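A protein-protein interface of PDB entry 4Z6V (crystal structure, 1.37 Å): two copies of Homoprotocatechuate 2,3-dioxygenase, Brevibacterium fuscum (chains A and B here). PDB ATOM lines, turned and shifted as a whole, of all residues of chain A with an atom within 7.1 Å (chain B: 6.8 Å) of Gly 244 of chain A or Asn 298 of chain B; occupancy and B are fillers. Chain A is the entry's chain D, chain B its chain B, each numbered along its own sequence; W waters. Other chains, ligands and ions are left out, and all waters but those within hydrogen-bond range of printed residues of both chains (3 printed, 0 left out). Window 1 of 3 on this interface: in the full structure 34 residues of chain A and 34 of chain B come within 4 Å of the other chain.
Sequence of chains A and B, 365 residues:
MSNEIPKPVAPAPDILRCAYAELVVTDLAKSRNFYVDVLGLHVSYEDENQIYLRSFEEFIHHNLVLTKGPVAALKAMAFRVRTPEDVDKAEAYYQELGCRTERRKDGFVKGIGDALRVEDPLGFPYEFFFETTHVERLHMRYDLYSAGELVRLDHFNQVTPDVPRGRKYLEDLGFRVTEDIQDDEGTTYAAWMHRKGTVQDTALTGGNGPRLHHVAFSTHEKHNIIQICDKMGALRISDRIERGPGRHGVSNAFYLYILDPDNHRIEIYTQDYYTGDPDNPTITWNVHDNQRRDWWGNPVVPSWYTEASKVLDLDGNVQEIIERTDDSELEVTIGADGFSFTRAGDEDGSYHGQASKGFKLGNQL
The side-chain amide nitrogen (ND2) of Asn 298 of chain B sits at hydrogen-bond distance from the backbone carbonyl oxygen (O) of Gly 244 of chain A (3.1 Å). The side-chain amino group (NZ) of Lys 357 of chain B is in hydrogen-bond range of the backbone carbonyl oxygen (O) of Ser 238 of chain A. NZ of Lys 357 of chain B lies within hydrogen-bond range of O of Ile 241 of chain A (2.9 Å).
Pro 245 of chain A touches Trp 296 of chain B, and with the chains exchanged Trp 296 of chain A touches Pro 245 of chain B. Of the 13 pairs that touch across the chains among the printed residues, 2 have their exchanged pair printed and touching as well.
Among the printed residues, pairs that only touch across the chains: Pro 245 of chain A with Trp 296 of chain B (3.2 Å), Cys 229 of chain A with Trp 296 of chain B (3.2 Å), Trp 296 of chain A with Pro 245 of chain B (3.3 Å), Ser 238 of chain A with Trp 296 of chain B (3.4 Å), Phe 359 of chain A with Val 301 of chain B (3.5 Å), Val 301 of chain A with Lys 357 of chain B (3.6 Å), Phe 359 of chain A with Pro 299 of chain B (3.6 Å), Ile 241 of chain A with Trp 296 of chain B (3.8 Å), Ser 238 of chain A with Trp 295 of chain B (3.9 Å) and Phe 359 of chain A with Val 300 of chain B (3.98 Å).
Of the 17 printed residues of chain A, 8 touch a printed residue of chain B. Hydrophobic or aromatic side chains of chain A within 4 Å of the printed part of chain B: Ile 241, Pro 245, Trp 296, Val 301 and Phe 359. Of the 16 printed residues of chain B, 8 touch a printed residue of chain A. Printed residues of chain B that touch a printed residue of chain A: Pro 245, Trp 295, Trp 296, Asn 298, Pro 299, Val 300, Val 301 and Lys 357. Hydrophobic or aromatic side chains of chain B that line the printed part of chain A: Pro 245, Trp 296, Pro 299 and Val 301. Among the printed residues, 13 pairs touch across the chains.
OD2 of Asp 294 of chain B sits close to N of Trp 296 of chain B, 3.2 Å away. The side-chain carboxylate of Asp 294 of chain B lies within hydrogen-bond range of the backbone NH of Asn 298 of chain B (3.0 Å). The backbone carbonyl oxygen (O) of Trp 296 of chain B sits at hydrogen-bond distance from the side-chain amino group (NZ) of Lys 357 of chain B (3.0 Å). The backbone NH (N) of Trp 296 of chain A lies close to the side-chain carboxylate (OD2) of Asp 294 of chain A, at 3.1 Å.
Printed residues of chain B within 4 Å of Cys 229 of chain A: Trp 296. Gly 244 of chain A touches just one residue of chain B: Asn 298. Of the printed residues of chain B, Val 301 of chain A touches Lys 357 (3.6 Å). Arg 243 of chain B touches none of the printed residues of chain A. No residue of chain A comes within 4 Å of Gly 297 of chain B. Of the printed residues of chain A, Asn 298 of chain B touches Gly 244 (3.1 Å). Of the printed residues of chain A, Pro 299 of chain B touches Phe 359. Ser 356 of chain B touches none of the printed residues of chain A. The nearest printed residue of chain A that does not touch Lys 357 of chain B is Glu 242 of chain A (4.002 Å).
Water W2 lies within hydrogen-bond range of the side-chain hydroxyl (OG) of Ser 238 of chain A (2.8 Å) and the side-chain amide nitrogen (ND2) of Asn 290 of chain B (2.9 Å). Water W3 lies within hydrogen-bond range of the backbone carbonyl oxygen (O) of Pro 245 of chain B (2.8 Å) and the backbone carbonyl oxygen (O) of Pro 245 of chain A (2.9 Å). Water W1 lies within hydrogen-bond range of the side-chain amide oxygen of Asn 298 of chain B (2.8 Å) and the backbone NH of Gly 244 of chain A (3.0 Å).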
ATOM      1  N   CYS A 229      12.964  11.299  15.946  1.00  0.00           N
ATOM      2  CA  CYS A 229      14.060  11.602  15.034  1.00  0.00           C
ATOM      3  C   CYS A 229      15.121  12.457  15.725  1.00  0.00           C
ATOM      4  O   CYS A 229      16.320  12.175  15.636  1.00  0.00           O
ATOM      5  CB  CYS A 229      13.566  12.355  13.779  1.00  0.00           C
ATOM      6  SG  CYS A 229      12.389  11.487  12.775  1.00  0.00           S
ATOM      7  N   SER A 238      21.407   8.303  14.030  1.00  0.00           N
ATOM      8  CA  SER A 238      20.587   8.710  12.883  1.00  0.00           C
ATOM      9  C   SER A 238      20.676   7.726  11.723  1.00  0.00           C
ATOM     10  O   SER A 238      19.805   7.721  10.859  1.00  0.00           O
ATOM     11  CB  SER A 238      20.949  10.102  12.383  1.00  0.00           C
ATOM     12  OG  SER A 238      22.312  10.213  12.008  1.00  0.00           O
ATOM     13  N   ILE A 241      17.639   5.629  11.427  1.00  0.00           N
ATOM     14  CA  ILE A 241      16.447   6.200  10.788  1.00  0.00           C
ATOM     15  C   ILE A 241      16.506   5.787   9.329  1.00  0.00           C
ATOM     16  O   ILE A 241      17.372   6.214   8.569  1.00  0.00           O
ATOM     17  CB  ILE A 241      16.366   7.729  10.920  1.00  0.00           C
ATOM     18  CG1 ILE A 241      16.378   8.178  12.381  1.00  0.00           C
ATOM     19  CG2 ILE A 241      15.156   8.286  10.189  1.00  0.00           C
ATOM     20  CD1 ILE A 241      16.561   9.696  12.495  1.00  0.00           C
ATOM     21  N   GLU A 242      15.599   4.910   8.950  1.00  0.00           N
ATOM     22  CA  GLU A 242      15.612   4.371   7.595  1.00  0.00           C
ATOM     23  C   GLU A 242      14.975   5.321   6.576  1.00  0.00           C
ATOM     24  O   GLU A 242      15.507   5.544   5.482  1.00  0.00           O
ATOM     25  CB  GLU A 242      14.922   3.018   7.532  1.00  0.00           C
ATOM     26  CG  GLU A 242      15.134   2.306   6.177  1.00  0.00           C
ATOM     27  CD  GLU A 242      14.189   1.134   5.938  1.00  0.00           C
ATOM     28  OE1 GLU A 242      13.061   1.161   6.480  1.00  0.00           O
ATOM     29  OE2 GLU A 242      14.573   0.200   5.201  1.00  0.00           O
ATOM     30  N   ARG A 243      13.778   5.798   6.918  1.00  0.00           N
ATOM     31  CA  ARG A 243      12.929   6.493   5.968  1.00  0.00           C
ATOM     32  C   ARG A 243      11.974   7.412   6.737  1.00  0.00           C
ATOM     33  O   ARG A 243      11.370   6.997   7.695  1.00  0.00           O
ATOM     34  CB  ARG A 243      12.133   5.509   5.127  1.00  0.00           C
ATOM     35  CG  ARG A 243      11.114   6.171   4.217  1.00  0.00           C
ATOM     36  CD  ARG A 243      10.375   5.179   3.319  1.00  0.00           C
ATOM     37  NE  ARG A 243       9.197   5.852   2.776  1.00  0.00           N
ATOM     38  CZ  ARG A 243       8.003   5.306   2.566  1.00  0.00           C
ATOM     39  NH1 ARG A 243       7.798   3.994   2.691  1.00  0.00           N
ATOM     40  NH2 ARG A 243       6.998   6.099   2.255  1.00  0.00           N
ATOM     41  N   GLY A 244      11.841   8.645   6.275  1.00  0.00           N
ATOM     42  CA  GLY A 244      10.962   9.620   6.887  1.00  0.00           C
ATOM     43  C   GLY A 244      11.709  10.692   7.642  1.00  0.00           C
ATOM     44  O   GLY A 244      12.925  10.852   7.490  1.00  0.00           O
ATOM     45  N   PRO A 245      10.983  11.470   8.450  1.00  0.00           N
ATOM     46  CA  PRO A 245       9.549  11.394   8.635  1.00  0.00           C
ATOM     47  C   PRO A 245       8.807  11.886   7.404  1.00  0.00           C
ATOM     48  O   PRO A 245       9.344  12.651   6.585  1.00  0.00           O
ATOM     49  CB  PRO A 245       9.307  12.296   9.839  1.00  0.00           C
ATOM     50  CG  PRO A 245      10.367  13.332   9.704  1.00  0.00           C
ATOM     51  CD  PRO A 245      11.566  12.618   9.160  1.00  0.00           C
ATOM     52  N   GLY A 246       7.560  11.473   7.266  1.00  0.00           N
ATOM     53  CA  GLY A 246       6.759  11.875   6.125  1.00  0.00           C
ATOM     54  C   GLY A 246       5.277  11.888   6.383  1.00  0.00           C
ATOM     55  O   GLY A 246       4.832  11.541   7.467  1.00  0.00           O
ATOM     56  N   TYR A 255       4.329   9.563   9.439  1.00  0.00           N
ATOM     57  CA  TYR A 255       5.066   8.322   9.611  1.00  0.00           C
ATOM     58  C   TYR A 255       6.569   8.484   9.749  1.00  0.00           C
ATOM     59  O   TYR A 255       7.150   9.508   9.367  1.00  0.00           O
ATOM     60  CB  TYR A 255       4.771   7.355   8.453  1.00  0.00           C
ATOM     61  CG  TYR A 255       5.470   7.723   7.180  1.00  0.00           C
ATOM     62  CD1 TYR A 255       6.755   7.277   6.927  1.00  0.00           C
ATOM     63  CD2 TYR A 255       4.865   8.527   6.234  1.00  0.00           C
ATOM     64  CE1 TYR A 255       7.429   7.652   5.768  1.00  0.00           C
ATOM     65  CE2 TYR A 255       5.514   8.878   5.062  1.00  0.00           C
ATOM     66  CZ  TYR A 255       6.794   8.425   4.826  1.00  0.00           C
ATOM     67  OH  TYR A 255       7.459   8.740   3.661  1.00  0.00           O
ATOM     68  N   LEU A 256       7.185   7.425  10.262  1.00  0.00           N
ATOM     69  CA  LEU A 256       8.632   7.287  10.336  1.00  0.00           C
ATOM     70  C   LEU A 256       8.974   5.803  10.358  1.00  0.00           C
ATOM     71  O   LEU A 256       8.256   5.046  11.011  1.00  0.00           O
ATOM     72  CB  LEU A 256       9.143   7.937  11.614  1.00  0.00           C
ATOM     73  CG  LEU A 256      10.625   7.797  11.943  1.00  0.00           C
ATOM     74  CD1 LEU A 256      11.417   8.650  10.979  1.00  0.00           C
ATOM     75  CD2 LEU A 256      10.868   8.205  13.375  1.00  0.00           C
ATOM     76  N   TYR A 257      10.069   5.408   9.708  1.00  0.00           N
ATOM     77  CA  TYR A 257      10.586   4.024   9.822  1.00  0.00           C
ATOM     78  C   TYR A 257      11.992   4.022  10.392  1.00  0.00           C
ATOM     79  O   TYR A 257      12.869   4.733   9.899  1.00  0.00           O
ATOM     80  CB  TYR A 257      10.605   3.314   8.487  1.00  0.00           C
ATOM     81  CG  TYR A 257       9.262   3.217   7.816  1.00  0.00           C
ATOM     82  CD1 TYR A 257       8.396   2.166   8.111  1.00  0.00           C
ATOM     83  CD2 TYR A 257       8.839   4.189   6.911  1.00  0.00           C
ATOM     84  CE1 TYR A 257       7.140   2.080   7.516  1.00  0.00           C
ATOM     85  CE2 TYR A 257       7.594   4.112   6.330  1.00  0.00           C
ATOM     86  CZ  TYR A 257       6.745   3.054   6.621  1.00  0.00           C
ATOM     87  OH  TYR A 257       5.512   3.009   6.010  1.00  0.00           O
ATOM     88  N   ASP A 294       4.942   8.542  -0.108  1.00  0.00           N
ATOM     89  CA  ASP A 294       5.218   9.801   0.559  1.00  0.00           C
ATOM     90  C   ASP A 294       4.480  10.882  -0.223  1.00  0.00           C
ATOM     91  O   ASP A 294       4.779  11.130  -1.394  1.00  0.00           O
ATOM     92  CB  ASP A 294       6.705  10.134   0.604  1.00  0.00           C
ATOM     93  CG  ASP A 294       6.964  11.335   1.496  1.00  0.00           C
ATOM     94  OD1 ASP A 294       7.007  11.141   2.749  1.00  0.00           O
ATOM     95  OD2 ASP A 294       7.090  12.463   0.929  1.00  0.00           O
ATOM     96  N   TRP A 296       4.504  13.964  -0.035  1.00  0.00           N
ATOM     97  CA  TRP A 296       5.332  15.125  -0.404  1.00  0.00           C
ATOM     98  C   TRP A 296       6.314  14.810  -1.519  1.00  0.00           C
ATOM     99  O   TRP A 296       7.139  15.658  -1.897  1.00  0.00           O
ATOM    100  CB  TRP A 296       6.096  15.584   0.838  1.00  0.00           C
ATOM    101  CG  TRP A 296       5.242  15.805   2.053  1.00  0.00           C
ATOM    102  CD1 TRP A 296       3.924  16.135   2.095  1.00  0.00           C
ATOM    103  CD2 TRP A 296       5.669  15.673   3.428  1.00  0.00           C
ATOM    104  NE1 TRP A 296       3.511  16.223   3.400  1.00  0.00           N
ATOM    105  CE2 TRP A 296       4.565  15.953   4.236  1.00  0.00           C
ATOM    106  CE3 TRP A 296       6.883  15.329   4.034  1.00  0.00           C
ATOM    107  CZ2 TRP A 296       4.648  15.924   5.642  1.00  0.00           C
ATOM    108  CZ3 TRP A 296       6.962  15.285   5.384  1.00  0.00           C
ATOM    109  CH2 TRP A 296       5.859  15.600   6.193  1.00  0.00           C
ATOM    110  N   ASN A 298       8.800  12.657  -1.453  1.00  0.00           N
ATOM    111  CA  ASN A 298      10.147  12.268  -1.093  1.00  0.00           C
ATOM    112  C   ASN A 298      10.415  10.833  -1.546  1.00  0.00           C
ATOM    113  O   ASN A 298       9.519   9.984  -1.540  1.00  0.00           O
ATOM    114  CB  ASN A 298      10.414  12.460   0.402  1.00  0.00           C
ATOM    115  CG  ASN A 298      10.768  13.892   0.746  1.00  0.00           C
ATOM    116  OD1 ASN A 298      11.406  14.585  -0.055  1.00  0.00           O
ATOM    117  ND2 ASN A 298      10.353  14.354   1.914  1.00  0.00           N
ATOM    118  N   PRO A 299      11.657  10.554  -1.938  1.00  0.00           N
ATOM    119  CA  PRO A 299      11.946   9.245  -2.499  1.00  0.00           C
ATOM    120  C   PRO A 299      11.864   8.130  -1.464  1.00  0.00           C
ATOM    121  O   PRO A 299      12.173   8.341  -0.291  1.00  0.00           O
ATOM    122  CB  PRO A 299      13.367   9.404  -3.063  1.00  0.00           C
ATOM    123  CG  PRO A 299      13.970  10.462  -2.221  1.00  0.00           C
ATOM    124  CD  PRO A 299      12.852  11.421  -1.932  1.00  0.00           C
ATOM    125  N   VAL A 301      13.386   4.979   0.027  1.00  0.00           N
ATOM    126  CA  VAL A 301      14.735   4.423   0.097  1.00  0.00           C
ATOM    127  C   VAL A 301      14.694   2.948  -0.361  1.00  0.00           C
ATOM    128  O   VAL A 301      13.755   2.212  -0.030  1.00  0.00           O
ATOM    129  CB  VAL A 301      15.311   4.563   1.517  1.00  0.00           C
ATOM    130  CG1 VAL A 301      15.264   6.018   2.006  1.00  0.00           C
ATOM    131  CG2 VAL A 301      14.623   3.672   2.510  1.00  0.00           C
ATOM    132  N   PHE A 359      18.014  12.069  -6.823  1.00  0.00           N
ATOM    133  CA  PHE A 359      18.807  10.890  -6.452  1.00  0.00           C
ATOM    134  C   PHE A 359      18.584   9.726  -7.414  1.00  0.00           C
ATOM    135  O   PHE A 359      17.466   9.527  -7.877  1.00  0.00           O
ATOM    136  CB  PHE A 359      18.433  10.444  -5.032  1.00  0.00           C
ATOM    137  CG  PHE A 359      18.789  11.453  -3.973  1.00  0.00           C
ATOM    138  CD1 PHE A 359      20.109  11.824  -3.767  1.00  0.00           C
ATOM    139  CD2 PHE A 359      17.789  12.032  -3.180  1.00  0.00           C
ATOM    140  CE1 PHE A 359      20.440  12.772  -2.792  1.00  0.00           C
ATOM    141  CE2 PHE A 359      18.107  12.962  -2.215  1.00  0.00           C
ATOM    142  CZ  PHE A 359      19.438  13.333  -2.016  1.00  0.00           C
ATOM    143  N   ARG B 243      13.573  20.064  -0.728  1.00  0.00           N
ATOM    144  CA  ARG B 243      14.314  19.394   0.335  1.00  0.00           C
ATOM    145  C   ARG B 243      13.602  19.593   1.668  1.00  0.00           C
ATOM    146  O   ARG B 243      13.175  20.699   2.004  1.00  0.00           O
ATOM    147  CB  ARG B 243      15.732  19.961   0.397  1.00  0.00           C
ATOM    148  CG  ARG B 243      16.542  19.480   1.589  1.00  0.00           C
ATOM    149  CD  ARG B 243      17.961  20.028   1.618  1.00  0.00           C
ATOM    150  NE  ARG B 243      18.512  19.749   2.942  1.00  0.00           N
ATOM    151  CZ  ARG B 243      19.264  20.558   3.672  1.00  0.00           C
ATOM    152  NH1 ARG B 243      19.797  21.656   3.132  1.00  0.00           N
ATOM    153  NH2 ARG B 243      19.544  20.225   4.930  1.00  0.00           N
ATOM    154  N   PRO B 245      10.751  18.066   4.808  1.00  0.00           N
ATOM    155  CA  PRO B 245      11.117  18.823   5.984  1.00  0.00           C
ATOM    156  C   PRO B 245      12.147  18.091   6.825  1.00  0.00           C
ATOM    157  O   PRO B 245      12.302  16.853   6.707  1.00  0.00           O
ATOM    158  CB  PRO B 245       9.778  18.969   6.721  1.00  0.00           C
ATOM    159  CG  PRO B 245       9.069  17.685   6.412  1.00  0.00           C
ATOM    160  CD  PRO B 245       9.453  17.382   4.976  1.00  0.00           C
ATOM    161  N   GLY B 246      12.866  18.855   7.644  1.00  0.00           N
ATOM    162  CA  GLY B 246      13.915  18.281   8.459  1.00  0.00           C
ATOM    163  C   GLY B 246      14.170  19.071   9.719  1.00  0.00           C
ATOM    164  O   GLY B 246      13.530  20.111   9.974  1.00  0.00           O
ATOM    165  N   TYR B 255      12.847  22.809   9.369  1.00  0.00           N
ATOM    166  CA  TYR B 255      12.991  23.499   8.083  1.00  0.00           C
ATOM    167  C   TYR B 255      12.326  22.797   6.914  1.00  0.00           C
ATOM    168  O   TYR B 255      12.035  21.590   6.979  1.00  0.00           O
ATOM    169  CB  TYR B 255      14.473  23.681   7.782  1.00  0.00           C
ATOM    170  CG  TYR B 255      15.174  22.399   7.325  1.00  0.00           C
ATOM    171  CD1 TYR B 255      15.177  22.003   5.995  1.00  0.00           C
ATOM    172  CD2 TYR B 255      15.824  21.590   8.235  1.00  0.00           C
ATOM    173  CE1 TYR B 255      15.787  20.814   5.589  1.00  0.00           C
ATOM    174  CE2 TYR B 255      16.481  20.421   7.843  1.00  0.00           C
ATOM    175  CZ  TYR B 255      16.445  20.022   6.524  1.00  0.00           C
ATOM    176  OH  TYR B 255      17.082  18.892   6.069  1.00  0.00           O
ATOM    177  N   ASN B 290      27.481  13.915   8.858  1.00  0.00           N
ATOM    178  CA  ASN B 290      26.213  13.743   8.181  1.00  0.00           C
ATOM    179  C   ASN B 290      24.980  14.202   8.978  1.00  0.00           C
ATOM    180  O   ASN B 290      23.865  14.147   8.441  1.00  0.00           O
ATOM    181  CB  ASN B 290      25.999  12.264   7.785  1.00  0.00           C
ATOM    182  CG  ASN B 290      24.852  12.088   6.809  1.00  0.00           C
ATOM    183  OD1 ASN B 290      24.817  12.717   5.744  1.00  0.00           O
ATOM    184  ND2 ASN B 290      23.896  11.243   7.166  1.00  0.00           N
ATOM    185  N   ARG B 293      23.675  19.227   8.430  1.00  0.00           N
ATOM    186  CA  ARG B 293      22.694  19.975   7.636  1.00  0.00           C
ATOM    187  C   ARG B 293      21.270  19.452   7.876  1.00  0.00           C
ATOM    188  O   ARG B 293      20.363  20.228   8.149  1.00  0.00           O
ATOM    189  CB  ARG B 293      23.055  19.970   6.155  1.00  0.00           C
ATOM    190  CG  ARG B 293      24.222  20.893   5.820  1.00  0.00           C
ATOM    191  CD  ARG B 293      24.253  21.256   4.359  1.00  0.00           C
ATOM    192  NE  ARG B 293      25.313  22.213   4.065  1.00  0.00           N
ATOM    193  CZ  ARG B 293      25.198  23.536   4.184  1.00  0.00           C
ATOM    194  NH1 ARG B 293      24.079  24.114   4.626  1.00  0.00           N
ATOM    195  NH2 ARG B 293      26.236  24.305   3.858  1.00  0.00           N
ATOM    196  N   ASP B 294      21.132  18.133   7.877  1.00  0.00           N
ATOM    197  CA  ASP B 294      19.945  17.443   8.363  1.00  0.00           C
ATOM    198  C   ASP B 294      20.389  16.552   9.528  1.00  0.00           C
ATOM    199  O   ASP B 294      21.174  15.613   9.344  1.00  0.00           O
ATOM    200  CB  ASP B 294      19.276  16.631   7.273  1.00  0.00           C
ATOM    201  CG  ASP B 294      17.948  16.084   7.735  1.00  0.00           C
ATOM    202  OD1 ASP B 294      16.972  16.875   7.717  1.00  0.00           O
ATOM    203  OD2 ASP B 294      17.886  14.912   8.185  1.00  0.00           O
ATOM    204  N   TRP B 295      19.914  16.892  10.718  1.00  0.00           N
ATOM    205  CA  TRP B 295      20.270  16.245  11.979  1.00  0.00           C
ATOM    206  C   TRP B 295      19.898  14.769  11.990  1.00  0.00           C
ATOM    207  O   TRP B 295      20.487  13.974  12.728  1.00  0.00           O
ATOM    208  CB  TRP B 295      19.527  16.989  13.082  1.00  0.00           C
ATOM    209  CG  TRP B 295      19.703  16.546  14.490  1.00  0.00           C
ATOM    210  CD1 TRP B 295      18.719  16.115  15.329  1.00  0.00           C
ATOM    211  CD2 TRP B 295      20.908  16.569  15.272  1.00  0.00           C
ATOM    212  NE1 TRP B 295      19.220  15.886  16.583  1.00  0.00           N
ATOM    213  CE2 TRP B 295      20.568  16.137  16.568  1.00  0.00           C
ATOM    214  CE3 TRP B 295      22.238  16.928  14.999  1.00  0.00           C
ATOM    215  CZ2 TRP B 295      21.503  16.091  17.611  1.00  0.00           C
ATOM    216  CZ3 TRP B 295      23.158  16.856  16.014  1.00  0.00           C
ATOM    217  CH2 TRP B 295      22.793  16.425  17.306  1.00  0.00           C
ATOM    218  N   TRP B 296      18.899  14.428  11.167  1.00  0.00           N
ATOM    219  CA  TRP B 296      18.401  13.058  11.081  1.00  0.00           C
ATOM    220  C   TRP B 296      19.186  12.236  10.040  1.00  0.00           C
ATOM    221  O   TRP B 296      18.908  11.048   9.794  1.00  0.00           O
ATOM    222  CB  TRP B 296      16.906  13.030  10.749  1.00  0.00           C
ATOM    223  CG  TRP B 296      16.074  13.880  11.640  1.00  0.00           C
ATOM    224  CD1 TRP B 296      16.327  14.224  12.945  1.00  0.00           C
ATOM    225  CD2 TRP B 296      14.864  14.551  11.277  1.00  0.00           C
ATOM    226  NE1 TRP B 296      15.328  15.056  13.431  1.00  0.00           N
ATOM    227  CE2 TRP B 296      14.422  15.278  12.422  1.00  0.00           C
ATOM    228  CE3 TRP B 296      14.118  14.621  10.098  1.00  0.00           C
ATOM    229  CZ2 TRP B 296      13.250  16.013  12.426  1.00  0.00           C
ATOM    230  CZ3 TRP B 296      12.964  15.367  10.105  1.00  0.00           C
ATOM    231  CH2 TRP B 296      12.532  16.043  11.260  1.00  0.00           C
ATOM    232  N   GLY B 297      20.168  12.892   9.425  1.00  0.00           N
ATOM    233  CA  GLY B 297      20.997  12.256   8.440  1.00  0.00           C
ATOM    234  C   GLY B 297      20.444  12.116   7.033  1.00  0.00           C
ATOM    235  O   GLY B 297      21.058  11.464   6.187  1.00  0.00           O
ATOM    236  N   ASN B 298      19.272  12.686   6.781  1.00  0.00           N
ATOM    237  CA  ASN B 298      18.732  12.653   5.442  1.00  0.00           C
ATOM    238  C   ASN B 298      19.682  13.335   4.459  1.00  0.00           C
ATOM    239  O   ASN B 298      20.334  14.324   4.788  1.00  0.00           O
ATOM    240  CB  ASN B 298      17.296  13.212   5.387  1.00  0.00           C
ATOM    241  CG  ASN B 298      16.278  12.207   5.889  1.00  0.00           C
ATOM    242  OD1 ASN B 298      16.424  11.013   5.656  1.00  0.00           O
ATOM    243  ND2 ASN B 298      15.237  12.686   6.557  1.00  0.00           N
ATOM    244  N   PRO B 299      19.760  12.805   3.225  1.00  0.00           N
ATOM    245  CA  PRO B 299      20.742  13.314   2.281  1.00  0.00           C
ATOM    246  C   PRO B 299      20.346  14.685   1.740  1.00  0.00           C
ATOM    247  O   PRO B 299      19.165  15.004   1.652  1.00  0.00           O
ATOM    248  CB  PRO B 299      20.734  12.260   1.169  1.00  0.00           C
ATOM    249  CG  PRO B 299      19.366  11.667   1.226  1.00  0.00           C
ATOM    250  CD  PRO B 299      19.041  11.634   2.689  1.00  0.00           C
ATOM    251  N   VAL B 300      21.335  15.505   1.422  1.00  0.00           N
ATOM    252  CA  VAL B 300      21.099  16.829   0.880  1.00  0.00           C
ATOM    253  C   VAL B 300      21.050  16.704  -0.633  1.00  0.00           C
ATOM    254  O   VAL B 300      22.019  16.296  -1.262  1.00  0.00           O
ATOM    255  CB  VAL B 300      22.179  17.843   1.329  1.00  0.00           C
ATOM    256  CG1 VAL B 300      21.919  19.205   0.696  1.00  0.00           C
ATOM    257  CG2 VAL B 300      22.206  17.963   2.847  1.00  0.00           C
ATOM    258  N   VAL B 301      19.903  17.068  -1.201  1.00  0.00           N
ATOM    259  CA  VAL B 301      19.682  16.944  -2.633  1.00  0.00           C
ATOM    260  C   VAL B 301      20.713  17.795  -3.411  1.00  0.00           C
ATOM    261  O   VAL B 301      21.024  18.917  -3.004  1.00  0.00           O
ATOM    262  CB  VAL B 301      18.222  17.301  -3.007  1.00  0.00           C
ATOM    263  CG1 VAL B 301      17.245  16.386  -2.275  1.00  0.00           C
ATOM    264  CG2 VAL B 301      17.909  18.738  -2.686  1.00  0.00           C
ATOM    265  N   SER B 356      23.783   9.509   1.972  1.00  0.00           N
ATOM    266  CA  SER B 356      23.171   8.671   3.002  1.00  0.00           C
ATOM    267  C   SER B 356      21.881   8.040   2.517  1.00  0.00           C
ATOM    268  O   SER B 356      21.320   8.433   1.472  1.00  0.00           O
ATOM    269  CB  SER B 356      22.865   9.517   4.237  1.00  0.00           C
ATOM    270  OG  SER B 356      22.072  10.635   3.878  1.00  0.00           O
ATOM    271  N   LYS B 357      21.425   7.068   3.302  1.00  0.00           N
ATOM    272  CA  LYS B 357      20.086   6.465   3.176  1.00  0.00           C
ATOM    273  C   LYS B 357      19.879   5.764   1.830  1.00  0.00           C
ATOM    274  O   LYS B 357      18.748   5.606   1.379  1.00  0.00           O
ATOM    275  CB  LYS B 357      18.955   7.500   3.377  1.00  0.00           C
ATOM    276  CG  LYS B 357      19.132   8.462   4.525  1.00  0.00           C
ATOM    277  CD  LYS B 357      18.714   7.909   5.857  1.00  0.00           C
ATOM    278  CE  LYS B 357      18.595   8.969   6.939  1.00  0.00           C
ATOM    279  NZ  LYS B 357      19.148   8.470   8.231  1.00  0.00           N
HETATM  280  O   HOH W   1      14.175   9.623   4.698  1.00  0.00           O
HETATM  281  O   HOH W   2      23.626   9.681   9.602  1.00  0.00           O
HETATM  282  O   HOH W   3      11.454  14.366   5.731  1.00  0.00           O
